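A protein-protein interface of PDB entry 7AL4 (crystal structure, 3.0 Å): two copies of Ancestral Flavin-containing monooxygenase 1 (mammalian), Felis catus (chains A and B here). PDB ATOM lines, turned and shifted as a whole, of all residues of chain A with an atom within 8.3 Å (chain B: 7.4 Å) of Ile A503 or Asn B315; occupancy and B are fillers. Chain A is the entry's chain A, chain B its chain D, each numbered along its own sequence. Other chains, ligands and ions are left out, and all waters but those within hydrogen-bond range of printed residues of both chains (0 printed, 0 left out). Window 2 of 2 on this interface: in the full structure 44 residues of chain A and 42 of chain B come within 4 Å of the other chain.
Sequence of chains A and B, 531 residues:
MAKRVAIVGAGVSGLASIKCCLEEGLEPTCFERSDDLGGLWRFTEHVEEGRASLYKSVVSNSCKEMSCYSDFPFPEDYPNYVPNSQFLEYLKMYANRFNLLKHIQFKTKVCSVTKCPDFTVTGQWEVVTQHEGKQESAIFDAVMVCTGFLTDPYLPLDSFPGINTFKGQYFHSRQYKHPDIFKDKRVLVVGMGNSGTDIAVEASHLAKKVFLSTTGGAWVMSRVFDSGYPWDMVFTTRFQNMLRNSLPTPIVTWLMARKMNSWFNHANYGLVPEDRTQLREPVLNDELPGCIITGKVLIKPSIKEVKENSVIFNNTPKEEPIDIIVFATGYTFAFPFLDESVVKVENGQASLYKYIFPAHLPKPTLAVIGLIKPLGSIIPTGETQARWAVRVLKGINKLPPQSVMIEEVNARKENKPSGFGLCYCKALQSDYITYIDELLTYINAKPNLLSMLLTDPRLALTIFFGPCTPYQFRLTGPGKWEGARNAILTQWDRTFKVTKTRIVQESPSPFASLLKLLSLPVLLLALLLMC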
ATOM      1  N   THR A 499      29.545  28.732  14.560  1.00  0.00           N
ATOM      2  CA  THR A 499      29.896  29.415  13.281  1.00  0.00           C
ATOM      3  C   THR A 499      28.943  28.918  12.187  1.00  0.00           C
ATOM      4  O   THR A 499      28.488  29.747  11.370  1.00  0.00           O
ATOM      5  CB  THR A 499      31.378  29.239  12.905  1.00  0.00           C
ATOM      6  OG1 THR A 499      31.655  27.888  12.544  1.00  0.00           O
ATOM      7  CG2 THR A 499      32.326  29.653  14.013  1.00  0.00           C
ATOM      8  N   LYS A 500      28.630  27.618  12.205  1.00  0.00           N
ATOM      9  CA  LYS A 500      27.819  26.915  11.169  1.00  0.00           C
ATOM     10  C   LYS A 500      26.327  27.143  11.432  1.00  0.00           C
ATOM     11  O   LYS A 500      25.597  26.141  11.575  1.00  0.00           O
ATOM     12  CB  LYS A 500      28.161  25.420  11.169  1.00  0.00           C
ATOM     13  CG  LYS A 500      27.504  24.582  10.080  1.00  0.00           C
ATOM     14  CD  LYS A 500      28.104  24.778   8.708  1.00  0.00           C
ATOM     15  CE  LYS A 500      27.749  23.663   7.744  1.00  0.00           C
ATOM     16  NZ  LYS A 500      28.449  22.393   8.073  1.00  0.00           N
ATOM     17  N   THR A 501      25.884  28.404  11.471  1.00  0.00           N
ATOM     18  CA  THR A 501      24.463  28.777  11.740  1.00  0.00           C
ATOM     19  C   THR A 501      23.630  28.575  10.474  1.00  0.00           C
ATOM     20  O   THR A 501      22.420  28.859  10.522  1.00  0.00           O
ATOM     21  CB  THR A 501      24.338  30.200  12.299  1.00  0.00           C
ATOM     22  OG1 THR A 501      25.336  30.999  11.662  1.00  0.00           O
ATOM     23  CG2 THR A 501      24.481  30.236  13.808  1.00  0.00           C
ATOM     24  N   ARG A 502      24.258  28.080   9.405  1.00  0.00           N
ATOM     25  CA  ARG A 502      23.591  27.783   8.109  1.00  0.00           C
ATOM     26  C   ARG A 502      24.186  26.517   7.477  1.00  0.00           C
ATOM     27  O   ARG A 502      25.345  26.559   6.999  1.00  0.00           O
ATOM     28  CB  ARG A 502      23.735  28.969   7.158  1.00  0.00           C
ATOM     29  CG  ARG A 502      22.831  28.888   5.939  1.00  0.00           C
ATOM     30  CD  ARG A 502      23.136  29.976   4.924  1.00  0.00           C
ATOM     31  NE  ARG A 502      24.005  29.522   3.836  1.00  0.00           N
ATOM     32  CZ  ARG A 502      23.618  29.289   2.582  1.00  0.00           C
ATOM     33  NH1 ARG A 502      22.356  29.475   2.221  1.00  0.00           N
ATOM     34  NH2 ARG A 502      24.498  28.871   1.692  1.00  0.00           N
ATOM     35  N   ILE A 503      23.390  25.445   7.463  1.00  0.00           N
ATOM     36  CA  ILE A 503      23.710  24.122   6.835  1.00  0.00           C
ATOM     37  C   ILE A 503      23.782  24.304   5.313  1.00  0.00           C
ATOM     38  O   ILE A 503      23.419  25.388   4.831  1.00  0.00           O
ATOM     39  CB  ILE A 503      22.686  23.036   7.238  1.00  0.00           C
ATOM     40  CG1 ILE A 503      21.338  23.166   6.511  1.00  0.00           C
ATOM     41  CG2 ILE A 503      22.520  22.971   8.753  1.00  0.00           C
ATOM     42  CD1 ILE A 503      20.662  24.523   6.590  1.00  0.00           C
ATOM     43  N   VAL A 504      24.217  23.266   4.594  1.00  0.00           N
ATOM     44  CA  VAL A 504      24.341  23.267   3.101  1.00  0.00           C
ATOM     45  C   VAL A 504      23.689  21.979   2.566  1.00  0.00           C
ATOM     46  O   VAL A 504      22.614  21.636   3.084  1.00  0.00           O
ATOM     47  CB  VAL A 504      25.813  23.487   2.687  1.00  0.00           C
ATOM     48  CG1 VAL A 504      26.724  22.322   3.054  1.00  0.00           C
ATOM     49  CG2 VAL A 504      25.956  23.883   1.222  1.00  0.00           C
ATOM     50  N   GLN A 505      24.273  21.301   1.572  1.00  0.00           N
ATOM     51  CA  GLN A 505      23.703  20.066   0.962  1.00  0.00           C
ATOM     52  C   GLN A 505      24.560  18.861   1.364  1.00  0.00           C
ATOM     53  O   GLN A 505      23.988  17.943   1.983  1.00  0.00           O
ATOM     54  CB  GLN A 505      23.627  20.208  -0.559  1.00  0.00           C
ATOM     55  CG  GLN A 505      23.129  21.576  -1.009  1.00  0.00           C
ATOM     56  CD  GLN A 505      22.573  21.577  -2.411  1.00  0.00           C
ATOM     57  OE1 GLN A 505      22.716  20.610  -3.160  1.00  0.00           O
ATOM     58  NE2 GLN A 505      21.931  22.674  -2.779  1.00  0.00           N
ATOM     59  N   ALA B 267      32.209  26.919   3.976  1.00  0.00           N
ATOM     60  CA  ALA B 267      31.232  25.862   4.348  1.00  0.00           C
ATOM     61  C   ALA B 267      30.922  25.942   5.849  1.00  0.00           C
ATOM     62  O   ALA B 267      29.719  25.979   6.208  1.00  0.00           O
ATOM     63  CB  ALA B 267      31.743  24.494   3.963  1.00  0.00           C
ATOM     64  N   GLY B 270      28.985  29.017   6.810  1.00  0.00           N
ATOM     65  CA  GLY B 270      27.629  28.923   6.234  1.00  0.00           C
ATOM     66  C   GLY B 270      27.423  29.941   5.138  1.00  0.00           C
ATOM     67  O   GLY B 270      26.283  30.397   4.988  1.00  0.00           O
ATOM     68  N   LEU B 271      28.494  30.279   4.411  1.00  0.00           N
ATOM     69  CA  LEU B 271      28.468  31.253   3.289  1.00  0.00           C
ATOM     70  C   LEU B 271      28.366  30.500   1.963  1.00  0.00           C
ATOM     71  O   LEU B 271      27.649  30.989   1.071  1.00  0.00           O
ATOM     72  CB  LEU B 271      29.720  32.130   3.351  1.00  0.00           C
ATOM     73  CG  LEU B 271      29.697  33.176   4.461  1.00  0.00           C
ATOM     74  CD1 LEU B 271      31.075  33.763   4.694  1.00  0.00           C
ATOM     75  CD2 LEU B 271      28.705  34.282   4.145  1.00  0.00           C
ATOM     76  N   VAL B 272      29.051  29.362   1.855  1.00  0.00           N
ATOM     77  CA  VAL B 272      29.093  28.511   0.626  1.00  0.00           C
ATOM     78  C   VAL B 272      27.817  28.721  -0.180  1.00  0.00           C
ATOM     79  O   VAL B 272      26.724  28.430   0.305  1.00  0.00           O
ATOM     80  CB  VAL B 272      29.269  27.017   0.949  1.00  0.00           C
ATOM     81  CG1 VAL B 272      30.733  26.659   1.150  1.00  0.00           C
ATOM     82  CG2 VAL B 272      28.415  26.581   2.132  1.00  0.00           C
ATOM     83  N   ILE B 299      25.284  34.333   9.975  1.00  0.00           N
ATOM     84  CA  ILE B 299      24.609  34.143   8.658  1.00  0.00           C
ATOM     85  C   ILE B 299      23.384  33.254   8.881  1.00  0.00           C
ATOM     86  O   ILE B 299      23.510  32.243   9.604  1.00  0.00           O
ATOM     87  CB  ILE B 299      25.583  33.553   7.623  1.00  0.00           C
ATOM     88  CG1 ILE B 299      26.811  34.448   7.447  1.00  0.00           C
ATOM     89  CG2 ILE B 299      24.888  33.285   6.295  1.00  0.00           C
ATOM     90  CD1 ILE B 299      28.104  33.680   7.444  1.00  0.00           C
ATOM     91  N   PRO B 301      19.902  31.364   6.719  1.00  0.00           N
ATOM     92  CA  PRO B 301      19.733  30.804   5.380  1.00  0.00           C
ATOM     93  C   PRO B 301      18.815  31.584   4.443  1.00  0.00           C
ATOM     94  O   PRO B 301      19.128  31.649   3.276  1.00  0.00           O
ATOM     95  CB  PRO B 301      19.093  29.431   5.604  1.00  0.00           C
ATOM     96  CG  PRO B 301      18.476  29.534   6.976  1.00  0.00           C
ATOM     97  CD  PRO B 301      19.359  30.482   7.758  1.00  0.00           C
ATOM     98  N   SER B 302      17.720  32.128   4.959  1.00  0.00           N
ATOM     99  CA  SER B 302      16.675  32.776   4.125  1.00  0.00           C
ATOM    100  C   SER B 302      15.468  33.071   5.000  1.00  0.00           C
ATOM    101  O   SER B 302      15.285  32.303   5.938  1.00  0.00           O
ATOM    102  CB  SER B 302      16.288  31.887   2.977  1.00  0.00           C
ATOM    103  OG  SER B 302      14.922  32.053   2.661  1.00  0.00           O
ATOM    104  N   LYS B 304      11.790  32.629   5.924  1.00  0.00           N
ATOM    105  CA  LYS B 304      10.655  31.694   5.681  1.00  0.00           C
ATOM    106  C   LYS B 304       9.346  32.468   5.857  1.00  0.00           C
ATOM    107  O   LYS B 304       8.508  32.433   4.940  1.00  0.00           O
ATOM    108  CB  LYS B 304      10.720  30.492   6.624  1.00  0.00           C
ATOM    109  CG  LYS B 304      10.135  29.209   6.048  1.00  0.00           C
ATOM    110  CD  LYS B 304       9.571  28.260   7.083  1.00  0.00           C
ATOM    111  CE  LYS B 304       9.218  26.905   6.504  1.00  0.00           C
ATOM    112  NZ  LYS B 304       8.073  26.292   7.220  1.00  0.00           N
ATOM    113  N   ILE B 312      11.292  33.988  11.072  1.00  0.00           N
ATOM    114  CA  ILE B 312      11.624  32.534  10.993  1.00  0.00           C
ATOM    115  C   ILE B 312      12.334  32.270   9.670  1.00  0.00           C
ATOM    116  O   ILE B 312      11.782  32.652   8.625  1.00  0.00           O
ATOM    117  CB  ILE B 312      10.375  31.648  11.138  1.00  0.00           C
ATOM    118  CG1 ILE B 312       9.505  32.087  12.322  1.00  0.00           C
ATOM    119  CG2 ILE B 312      10.789  30.183  11.233  1.00  0.00           C
ATOM    120  CD1 ILE B 312       8.154  31.407  12.404  1.00  0.00           C
ATOM    121  N   PHE B 313      13.494  31.611   9.739  1.00  0.00           N
ATOM    122  CA  PHE B 313      14.355  31.285   8.575  1.00  0.00           C
ATOM    123  C   PHE B 313      14.097  29.831   8.161  1.00  0.00           C
ATOM    124  O   PHE B 313      13.763  29.015   9.032  1.00  0.00           O
ATOM    125  CB  PHE B 313      15.822  31.585   8.901  1.00  0.00           C
ATOM    126  CG  PHE B 313      16.062  32.961   9.470  1.00  0.00           C
ATOM    127  CD1 PHE B 313      16.163  34.067   8.645  1.00  0.00           C
ATOM    128  CD2 PHE B 313      16.191  33.154  10.836  1.00  0.00           C
ATOM    129  CE1 PHE B 313      16.377  35.329   9.175  1.00  0.00           C
ATOM    130  CE2 PHE B 313      16.412  34.417  11.365  1.00  0.00           C
ATOM    131  CZ  PHE B 313      16.497  35.504  10.534  1.00  0.00           C
ATOM    132  N   ASN B 314      14.218  29.540   6.862  1.00  0.00           N
ATOM    133  CA  ASN B 314      14.082  28.174   6.276  1.00  0.00           C
ATOM    134  C   ASN B 314      15.142  27.262   6.908  1.00  0.00           C
ATOM    135  O   ASN B 314      16.207  27.776   7.275  1.00  0.00           O
ATOM    136  CB  ASN B 314      14.227  28.180   4.751  1.00  0.00           C
ATOM    137  CG  ASN B 314      13.146  28.981   4.064  1.00  0.00           C
ATOM    138  OD1 ASN B 314      12.196  28.413   3.533  1.00  0.00           O
ATOM    139  ND2 ASN B 314      13.274  30.298   4.078  1.00  0.00           N
ATOM    140  N   ASN B 315      14.856  25.964   7.047  1.00  0.00           N
ATOM    141  CA  ASN B 315      15.819  24.965   7.598  1.00  0.00           C
ATOM    142  C   ASN B 315      16.390  25.456   8.937  1.00  0.00           C
ATOM    143  O   ASN B 315      17.513  25.032   9.303  1.00  0.00           O
ATOM    144  CB  ASN B 315      16.998  24.702   6.651  1.00  0.00           C
ATOM    145  CG  ASN B 315      16.580  24.300   5.252  1.00  0.00           C
ATOM    146  OD1 ASN B 315      15.449  24.552   4.836  1.00  0.00           O
ATOM    147  ND2 ASN B 315      17.490  23.676   4.522  1.00  0.00           N
ATOM    148  N   THR B 316      15.651  26.325   9.629  1.00  0.00           N
ATOM    149  CA  THR B 316      16.099  27.001  10.877  1.00  0.00           C
ATOM    150  C   THR B 316      14.985  26.894  11.908  1.00  0.00           C
ATOM    151  O   THR B 316      13.999  27.633  11.845  1.00  0.00           O
ATOM    152  CB  THR B 316      16.532  28.444  10.600  1.00  0.00           C
ATOM    153  OG1 THR B 316      17.775  28.360   9.902  1.00  0.00           O
ATOM    154  CG2 THR B 316      16.696  29.287  11.847  1.00  0.00           C
ATOM    155  N   PRO B 317      15.120  25.967  12.884  1.00  0.00           N
ATOM    156  CA  PRO B 317      14.061  25.730  13.862  1.00  0.00           C
ATOM    157  C   PRO B 317      13.840  26.955  14.760  1.00  0.00           C
ATOM    158  O   PRO B 317      12.687  27.273  14.995  1.00  0.00           O
ATOM    159  CB  PRO B 317      14.558  24.508  14.644  1.00  0.00           C
ATOM    160  CG  PRO B 317      16.065  24.549  14.498  1.00  0.00           C
ATOM    161  CD  PRO B 317      16.306  25.123  13.119  1.00  0.00           C
ATOM    162  N   LYS B 318      14.923  27.626  15.180  1.00  0.00           N
ATOM    163  CA  LYS B 318      14.858  28.783  16.120  1.00  0.00           C
ATOM    164  C   LYS B 318      14.219  29.997  15.425  1.00  0.00           C
ATOM    165  O   LYS B 318      14.778  30.502  14.414  1.00  0.00           O
ATOM    166  CB  LYS B 318      16.224  29.151  16.705  1.00  0.00           C
ATOM    167  CG  LYS B 318      16.142  29.921  18.021  1.00  0.00           C
ATOM    168  CD  LYS B 318      17.423  30.613  18.439  1.00  0.00           C
ATOM    169  CE  LYS B 318      18.597  29.670  18.575  1.00  0.00           C
ATOM    170  NZ  LYS B 318      19.783  30.361  19.132  1.00  0.00           N
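Ala B267 touches Lys A500 (O to CD, 3.2 Å). Arg A502 touches Leu B271 (NH2 to O, 3.8 Å). Arg A502 touches Ile B299. Arg A502 touches Pro B301. CB of Asn B315 touches CD1 of Ile A503, 3.7 Å away. CG2 of Val A504 touches CG2 of Val B272, at 3.8 Å.
The backbone carbonyl oxygen (O) of Ile B299 lies within hydrogen-bond range of the side-chain hydroxyl (OG1) of Thr A501, 3.0 Å away. NE of Arg A502 lies within hydrogen-bond range of O of Gly B270 (2.7 Å). The backbone carbonyl oxygen (O) of Val B272 lies within hydrogen-bond range of the guanidinium group (NH2) of Arg A502.
Hydrophobic or aromatic side chains of chain B within 4 Å of the printed part of chain A: Val B272, Ile B299 and Pro B301. Of the 7 printed residues of chain A, 5 touch a printed residue of chain B. Hydrophobic or aromatic side chains of chain A within 4 Å of the printed part of chain B: Ile A503 and Val A504. Among the printed residues, 9 pairs touch across the chains. Among the printed residues, no Asp or Glu carboxylate lies within 4 Å of a Lys or Arg side-chain nitrogen of the other chain.
OG1 of Thr A501 lies within hydrogen-bond range of O of Thr A499, at 3.4 Å.
Of chain B, only Asn B315 (3.7 Å) comes within 4 Å of Ile A503. Of the printed residues of chain A, Asn B315 touches Ile A503 (3.7 Å). Printed residues of chain A within 4 Å of Leu B271: Arg A502. Printed residues of chain A within 4 Å of Val B272: Arg A502 and Val A504. Of the printed residues of chain B, Arg A502 touches Gly B270 (2.7 Å), Leu B271 (3.8 Å), Val B272 (2.7 Å), Ile B299 (3.99 Å) and Pro B301 (3.5 Å). Of the printed residues of chain B, Lys A500 touches Ala B267. Of the printed residues of chain A, Gly B270 touches Arg A502. The nearest residue of chain B that does not touch Ile A503 is Pro B301 (5.2 Å). The nearest printed residue of chain A that does not touch Leu B271 is Thr A499 (7.0 Å).
No position is printed for both chains. Of the 9 pairs that touch across the chains among the printed residues, none has its exchanged pair printed and touching as well.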
